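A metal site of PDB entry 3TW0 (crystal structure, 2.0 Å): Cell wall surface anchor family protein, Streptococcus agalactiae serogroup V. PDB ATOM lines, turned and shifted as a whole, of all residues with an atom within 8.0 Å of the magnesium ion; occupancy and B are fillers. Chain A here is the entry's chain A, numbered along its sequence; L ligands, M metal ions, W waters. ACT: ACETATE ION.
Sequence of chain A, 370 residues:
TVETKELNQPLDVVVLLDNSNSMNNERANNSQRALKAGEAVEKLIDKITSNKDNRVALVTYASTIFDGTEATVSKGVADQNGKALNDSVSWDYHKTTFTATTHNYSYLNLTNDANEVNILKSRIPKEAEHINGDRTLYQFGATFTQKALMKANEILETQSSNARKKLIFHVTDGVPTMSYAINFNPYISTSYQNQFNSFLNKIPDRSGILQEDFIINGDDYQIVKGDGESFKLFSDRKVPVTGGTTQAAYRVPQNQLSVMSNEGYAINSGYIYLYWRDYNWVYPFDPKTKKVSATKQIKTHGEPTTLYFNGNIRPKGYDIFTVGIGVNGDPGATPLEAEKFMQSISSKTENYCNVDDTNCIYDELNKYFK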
ATOM      1  N   ASP A  18       4.104  10.444  -9.789  1.00  0.00           N
ATOM      2  CA  ASP A  18       3.216  11.530 -10.202  1.00  0.00           C
ATOM      3  C   ASP A  18       2.012  11.569  -9.224  1.00  0.00           C
ATOM      4  O   ASP A  18       1.287  10.593  -9.072  1.00  0.00           O
ATOM      5  CB  ASP A  18       2.781  11.215 -11.658  1.00  0.00           C
ATOM      6  CG  ASP A  18       1.843  12.259 -12.275  1.00  0.00           C
ATOM      7  OD1 ASP A  18       1.252  13.103 -11.563  1.00  0.00           O
ATOM      8  OD2 ASP A  18       1.654  12.207 -13.524  1.00  0.00           O
ATOM      9  N   ASN A  19       1.872  12.677  -8.493  1.00  0.00           N
ATOM     10  CA  ASN A  19       0.746  12.841  -7.583  1.00  0.00           C
ATOM     11  C   ASN A  19      -0.046  14.074  -7.998  1.00  0.00           C
ATOM     12  O   ASN A  19      -0.638  14.774  -7.165  1.00  0.00           O
ATOM     13  CB  ASN A  19       1.243  12.961  -6.130  1.00  0.00           C
ATOM     14  CG  ASN A  19       0.122  12.799  -5.052  1.00  0.00           C
ATOM     15  OD1 ASN A  19      -0.684  11.855  -5.080  1.00  0.00           O
ATOM     16  ND2 ASN A  19       0.144  13.684  -4.095  1.00  0.00           N
ATOM     17  N   SER A  20      -0.041  14.372  -9.298  1.00  0.00           N
ATOM     18  CA  SER A  20      -0.801  15.510  -9.763  1.00  0.00           C
ATOM     19  C   SER A  20      -2.349  15.314  -9.625  1.00  0.00           C
ATOM     20  O   SER A  20      -2.825  14.199  -9.399  1.00  0.00           O
ATOM     21  CB  SER A  20      -0.390  15.890 -11.180  1.00  0.00           C
ATOM     22  OG  SER A  20      -0.630  14.837 -12.091  1.00  0.00           O
ATOM     23  N   ASN A  21      -3.101  16.402  -9.756  1.00  0.00           N
ATOM     24  CA  ASN A  21      -4.564  16.348  -9.660  1.00  0.00           C
ATOM     25  C   ASN A  21      -5.204  15.389 -10.657  1.00  0.00           C
ATOM     26  O   ASN A  21      -6.213  14.729 -10.344  1.00  0.00           O
ATOM     27  CB  ASN A  21      -5.175  17.735  -9.836  1.00  0.00           C
ATOM     28  CG  ASN A  21      -4.758  18.665  -8.737  1.00  0.00           C
ATOM     29  OD1 ASN A  21      -4.367  18.237  -7.642  1.00  0.00           O
ATOM     30  ND2 ASN A  21      -4.804  19.968  -9.026  1.00  0.00           N
ATOM     31  N   SER A  22      -4.604  15.288 -11.854  1.00  0.00           N
ATOM     32  CA  SER A  22      -5.109  14.339 -12.871  1.00  0.00           C
ATOM     33  C   SER A  22      -5.050  12.896 -12.339  1.00  0.00           C
ATOM     34  O   SER A  22      -5.732  12.000 -12.884  1.00  0.00           O
ATOM     35  CB  SER A  22      -4.348  14.477 -14.192  1.00  0.00           C
ATOM     36  OG  SER A  22      -2.991  14.020 -14.075  1.00  0.00           O
ATOM     37  N   MET A  23      -4.265  12.666 -11.277  1.00  0.00           N
ATOM     38  CA  MET A  23      -4.142  11.315 -10.752  1.00  0.00           C
ATOM     39  C   MET A  23      -5.230  11.005  -9.699  1.00  0.00           C
ATOM     40  O   MET A  23      -5.331   9.872  -9.260  1.00  0.00           O
ATOM     41  CB  MET A  23      -2.747  11.065 -10.142  1.00  0.00           C
ATOM     42  CG  MET A  23      -1.586  11.233 -11.120  1.00  0.00           C
ATOM     43  SD  MET A  23      -1.417   9.880 -12.296  1.00  0.00           S
ATOM     44  CE  MET A  23      -0.845   8.570 -11.248  1.00  0.00           C
ATOM     45  N   ASN A  24      -6.013  12.008  -9.287  1.00  0.00           N
ATOM     46  CA  ASN A  24      -7.136  11.757  -8.351  1.00  0.00           C
ATOM     47  C   ASN A  24      -7.941  10.522  -8.789  1.00  0.00           C
ATOM     48  O   ASN A  24      -8.214  10.331  -9.987  1.00  0.00           O
ATOM     49  CB  ASN A  24      -8.020  12.987  -8.191  1.00  0.00           C
ATOM     50  CG  ASN A  24      -9.235  12.732  -7.290  1.00  0.00           C
ATOM     51  OD1 ASN A  24     -10.261  12.220  -7.730  1.00  0.00           O
ATOM     52  ND2 ASN A  24      -9.118  13.086  -6.023  1.00  0.00           N
ATOM     53  N   ARG A  27     -10.886  10.624 -11.376  1.00  0.00           N
ATOM     54  CA  ARG A  27     -10.612  11.030 -12.782  1.00  0.00           C
ATOM     55  C   ARG A  27     -10.705   9.878 -13.768  1.00  0.00           C
ATOM     56  O   ARG A  27     -10.529   8.713 -13.399  1.00  0.00           O
ATOM     57  CB  ARG A  27      -9.213  11.669 -12.945  1.00  0.00           C
ATOM     58  CG  ARG A  27      -8.974  12.959 -12.169  1.00  0.00           C
ATOM     59  CD  ARG A  27      -9.724  14.147 -12.813  1.00  0.00           C
ATOM     60  NE  ARG A  27      -9.446  15.412 -12.126  1.00  0.00           N
ATOM     61  CZ  ARG A  27      -8.619  16.352 -12.595  1.00  0.00           C
ATOM     62  NH1 ARG A  27      -7.990  16.206 -13.762  1.00  0.00           N
ATOM     63  NH2 ARG A  27      -8.455  17.462 -11.891  1.00  0.00           N
ATOM     64  N   ARG A  33      -6.293   6.180 -10.586  1.00  0.00           N
ATOM     65  CA  ARG A  33      -4.911   6.430 -10.957  1.00  0.00           C
ATOM     66  C   ARG A  33      -3.967   6.399  -9.758  1.00  0.00           C
ATOM     67  O   ARG A  33      -3.027   5.621  -9.740  1.00  0.00           O
ATOM     68  CB  ARG A  33      -4.818   7.732 -11.739  1.00  0.00           C
ATOM     69  CG  ARG A  33      -5.178   7.587 -13.203  1.00  0.00           C
ATOM     70  CD  ARG A  33      -5.067   8.901 -13.866  1.00  0.00           C
ATOM     71  NE  ARG A  33      -5.359   8.801 -15.283  1.00  0.00           N
ATOM     72  CZ  ARG A  33      -5.944   9.762 -15.990  1.00  0.00           C
ATOM     73  NH1 ARG A  33      -6.312  10.891 -15.407  1.00  0.00           N
ATOM     74  NH2 ARG A  33      -6.172   9.570 -17.304  1.00  0.00           N
ATOM     75  N   TYR A  61       5.783  13.895  -6.762  1.00  0.00           N
ATOM     76  CA  TYR A  61       5.760  15.233  -7.331  1.00  0.00           C
ATOM     77  C   TYR A  61       4.437  15.595  -7.901  1.00  0.00           C
ATOM     78  O   TYR A  61       3.617  14.733  -8.250  1.00  0.00           O
ATOM     79  CB  TYR A  61       6.798  15.384  -8.453  1.00  0.00           C
ATOM     80  CG  TYR A  61       6.449  14.699  -9.765  1.00  0.00           C
ATOM     81  CD1 TYR A  61       5.816  15.401 -10.795  1.00  0.00           C
ATOM     82  CD2 TYR A  61       6.841  13.362 -10.026  1.00  0.00           C
ATOM     83  CE1 TYR A  61       5.513  14.791 -12.005  1.00  0.00           C
ATOM     84  CE2 TYR A  61       6.563  12.752 -11.268  1.00  0.00           C
ATOM     85  CZ  TYR A  61       5.880  13.474 -12.249  1.00  0.00           C
ATOM     86  OH  TYR A  61       5.566  12.921 -13.494  1.00  0.00           O
ATOM     87  N   ALA A  62       4.253  16.889  -8.014  1.00  0.00           N
ATOM     88  CA  ALA A  62       3.175  17.442  -8.783  1.00  0.00           C
ATOM     89  C   ALA A  62       3.678  18.778  -9.307  1.00  0.00           C
ATOM     90  O   ALA A  62       4.609  18.774 -10.114  1.00  0.00           O
ATOM     91  CB  ALA A  62       1.896  17.529  -7.958  1.00  0.00           C
ATOM     92  N   GLY A 141      -1.142  21.064  -7.726  1.00  0.00           N
ATOM     93  CA  GLY A 141      -1.438  19.773  -8.374  1.00  0.00           C
ATOM     94  C   GLY A 141      -1.158  19.691  -9.870  1.00  0.00           C
ATOM     95  O   GLY A 141      -1.667  18.814 -10.532  1.00  0.00           O
ATOM     96  N   ALA A 142      -0.327  20.590 -10.390  1.00  0.00           N
ATOM     97  CA  ALA A 142       0.151  20.462 -11.802  1.00  0.00           C
ATOM     98  C   ALA A 142       1.097  19.255 -12.003  1.00  0.00           C
ATOM     99  O   ALA A 142       1.474  18.596 -11.063  1.00  0.00           O
ATOM    100  CB  ALA A 142       0.817  21.772 -12.246  1.00  0.00           C
ATOM    101  N   THR A 143       1.480  18.967 -13.253  1.00  0.00           N
ATOM    102  CA  THR A 143       2.360  17.817 -13.517  1.00  0.00           C
ATOM    103  C   THR A 143       3.731  18.334 -13.988  1.00  0.00           C
ATOM    104  O   THR A 143       3.980  18.467 -15.186  1.00  0.00           O
ATOM    105  CB  THR A 143       1.707  16.853 -14.522  1.00  0.00           C
ATOM    106  OG1 THR A 143       0.337  16.645 -14.142  1.00  0.00           O
ATOM    107  CG2 THR A 143       2.427  15.480 -14.563  1.00  0.00           C
ATOM    108  N   PHE A 144       4.583  18.725 -13.051  1.00  0.00           N
ATOM    109  CA  PHE A 144       5.870  19.318 -13.392  1.00  0.00           C
ATOM    110  C   PHE A 144       6.892  18.164 -13.466  1.00  0.00           C
ATOM    111  O   PHE A 144       7.785  18.064 -12.640  1.00  0.00           O
ATOM    112  CB  PHE A 144       6.293  20.354 -12.332  1.00  0.00           C
ATOM    113  CG  PHE A 144       7.346  21.324 -12.811  1.00  0.00           C
ATOM    114  CD1 PHE A 144       7.993  21.139 -14.031  1.00  0.00           C
ATOM    115  CD2 PHE A 144       7.717  22.388 -12.004  1.00  0.00           C
ATOM    116  CE1 PHE A 144       8.963  22.054 -14.460  1.00  0.00           C
ATOM    117  CE2 PHE A 144       8.693  23.311 -12.435  1.00  0.00           C
ATOM    118  CZ  PHE A 144       9.301  23.159 -13.661  1.00  0.00           C
ATOM    119  N   THR A 145       6.677  17.270 -14.400  1.00  0.00           N
ATOM    120  CA  THR A 145       7.597  16.167 -14.668  1.00  0.00           C
ATOM    121  C   THR A 145       9.070  16.560 -14.780  1.00  0.00           C
ATOM    122  O   THR A 145       9.921  15.876 -14.223  1.00  0.00           O
ATOM    123  CB  THR A 145       7.104  15.383 -15.915  1.00  0.00           C
ATOM    124  OG1 THR A 145       5.793  14.857 -15.642  1.00  0.00           O
ATOM    125  CG2 THR A 145       8.020  14.185 -16.231  1.00  0.00           C
ATOM    126  N   THR A 172       3.175   7.401 -13.732  1.00  0.00           N
ATOM    127  CA  THR A 172       2.501   8.644 -14.115  1.00  0.00           C
ATOM    128  C   THR A 172       1.398   8.349 -15.115  1.00  0.00           C
ATOM    129  O   THR A 172       1.357   7.254 -15.684  1.00  0.00           O
ATOM    130  CB  THR A 172       3.547   9.640 -14.725  1.00  0.00           C
ATOM    131  OG1 THR A 172       2.920  10.826 -15.209  1.00  0.00           O
ATOM    132  CG2 THR A 172       4.342   8.980 -15.869  1.00  0.00           C
ATOM    133  N   ASP A 173       0.503   9.293 -15.334  1.00  0.00           N
ATOM    134  CA  ASP A 173      -0.467   9.155 -16.425  1.00  0.00           C
ATOM    135  C   ASP A 173       0.056   9.788 -17.738  1.00  0.00           C
ATOM    136  O   ASP A 173      -0.625   9.762 -18.760  1.00  0.00           O
ATOM    137  CB  ASP A 173      -1.863   9.693 -16.023  1.00  0.00           C
ATOM    138  CG  ASP A 173      -1.856  11.184 -15.732  1.00  0.00           C
ATOM    139  OD1 ASP A 173      -0.944  11.886 -16.226  1.00  0.00           O
ATOM    140  OD2 ASP A 173      -2.761  11.676 -15.055  1.00  0.00           O
ATOM    141  N   GLY A 174       1.273  10.326 -17.678  1.00  0.00           N
ATOM    142  CA  GLY A 174       1.987  10.768 -18.880  1.00  0.00           C
ATOM    143  C   GLY A 174       1.637  12.115 -19.474  1.00  0.00           C
ATOM    144  O   GLY A 174       1.894  12.366 -20.662  1.00  0.00           O
ATOM    145  N   VAL A 175       1.049  13.016 -18.684  1.00  0.00           N
ATOM    146  CA  VAL A 175       0.652  14.329 -19.246  1.00  0.00           C
ATOM    147  C   VAL A 175       1.244  15.489 -18.476  1.00  0.00           C
ATOM    148  O   VAL A 175       0.624  15.982 -17.504  1.00  0.00           O
ATOM    149  CB  VAL A 175      -0.884  14.494 -19.370  1.00  0.00           C
ATOM    150  CG1 VAL A 175      -1.233  15.803 -20.088  1.00  0.00           C
ATOM    151  CG2 VAL A 175      -1.523  13.279 -20.092  1.00  0.00           C
ATOM    152  N   PRO A 176       2.452  15.938 -18.858  1.00  0.00           N
ATOM    153  CA  PRO A 176       3.048  17.056 -18.139  1.00  0.00           C
ATOM    154  C   PRO A 176       2.382  18.351 -18.536  1.00  0.00           C
ATOM    155  O   PRO A 176       2.012  18.540 -19.704  1.00  0.00           O
ATOM    156  CB  PRO A 176       4.510  17.031 -18.587  1.00  0.00           C
ATOM    157  CG  PRO A 176       4.429  16.508 -20.029  1.00  0.00           C
ATOM    158  CD  PRO A 176       3.333  15.473 -19.975  1.00  0.00           C
ATOM    159  N   THR A 177       2.227  19.251 -17.563  1.00  0.00           N
ATOM    160  CA  THR A 177       1.451  20.467 -17.757  1.00  0.00           C
ATOM    161  C   THR A 177       2.182  21.661 -17.159  1.00  0.00           C
ATOM    162  O   THR A 177       1.603  22.724 -16.941  1.00  0.00           O
ATOM    163  CB  THR A 177       0.091  20.353 -17.041  1.00  0.00           C
ATOM    164  OG1 THR A 177       0.329  20.093 -15.650  1.00  0.00           O
ATOM    165  CG2 THR A 177      -0.761  19.217 -17.606  1.00  0.00           C
ATOM    166  N   GLY A 228      -0.543  23.858 -14.790  1.00  0.00           N
ATOM    167  CA  GLY A 228      -1.435  22.702 -14.695  1.00  0.00           C
ATOM    168  C   GLY A 228      -2.716  22.725 -15.552  1.00  0.00           C
ATOM    169  O   GLY A 228      -3.475  21.787 -15.543  1.00  0.00           O
ATOM    170  N   ASP A 330      -5.480  13.520 -20.205  1.00  0.00           N
ATOM    171  CA  ASP A 330      -6.036  14.604 -19.382  1.00  0.00           C
ATOM    172  C   ASP A 330      -4.929  15.390 -18.625  1.00  0.00           C
ATOM    173  O   ASP A 330      -4.097  14.774 -17.960  1.00  0.00           O
ATOM    174  CB  ASP A 330      -7.104  14.053 -18.412  1.00  0.00           C
ATOM    175  CG  ASP A 330      -7.842  15.161 -17.595  1.00  0.00           C
ATOM    176  OD1 ASP A 330      -8.126  16.272 -18.120  1.00  0.00           O
ATOM    177  OD2 ASP A 330      -8.178  14.893 -16.419  1.00  0.00           O
ATOM    178  N   PRO A 331      -4.895  16.735 -18.774  1.00  0.00           N
ATOM    179  CA  PRO A 331      -5.674  17.602 -19.704  1.00  0.00           C
ATOM    180  C   PRO A 331      -4.923  18.034 -20.988  1.00  0.00           C
ATOM    181  O   PRO A 331      -3.728  18.330 -20.936  1.00  0.00           O
ATOM    182  CB  PRO A 331      -5.908  18.848 -18.859  1.00  0.00           C
ATOM    183  CG  PRO A 331      -4.587  18.981 -18.087  1.00  0.00           C
ATOM    184  CD  PRO A 331      -4.128  17.547 -17.808  1.00  0.00           C
HETATM  185  C   ACT L   1      -2.487  18.127 -13.578  1.00  0.00           C
HETATM  186  O   ACT L   1      -2.483  16.901 -13.359  1.00  0.00           O
HETATM  187  OXT ACT L   1      -1.494  18.543 -14.219  1.00  0.00           O
HETATM  188  CH3 ACT L   1      -3.587  19.054 -13.088  1.00  0.00           C
HETATM  189 MG    MG M   1      -1.260  15.290 -13.915  1.00  0.00          MG
HETATM  190  O   HOH W   1      -0.323  13.703 -14.481  1.00  0.00           O
HETATM  191  O   HOH W   2      -1.715  15.716 -16.041  1.00  0.00           O
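NH1 of Arg 33 lies within hydrogen-bond range of O of Ser 22, 2.8 Å away. OG1 of Thr 177 lies within hydrogen-bond range of N of Thr 143. The side-chain carboxylate (OD2) of Asp 173 sits close to the side-chain hydroxyl (OG) of Ser 22 (2.6 Å). The side-chain hydroxyl of Thr 143 lies close to the backbone carbonyl oxygen of Val 175 (3.4 Å). OD1 of Asp 18 lies within hydrogen-bond range of N of Ser 20 (2.9 Å).
Within 4 Å of the magnesium ion: Ser 20, Ser 22 and Thr 143.
The magnesium ion is bound by water W1 (1.9 Å), OG of Ser 20 (2.0 Å), O of the ligand (2.1 Å), OG1 of Thr 143 (2.1 Å), OG of Ser 22 (2.2 Å) and water W2 (2.2 Å). The magnesium ion has six donor atoms within binding distance.
Water W1 lies within hydrogen-bond range of the side-chain carboxylate of Asp 173 (2.6 Å) and the side-chain carboxylate of Asp 18 (2.7 Å). Water W2 bridges O of Val 175 (2.8 Å) and O of Asp 330 (3.2 Å).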
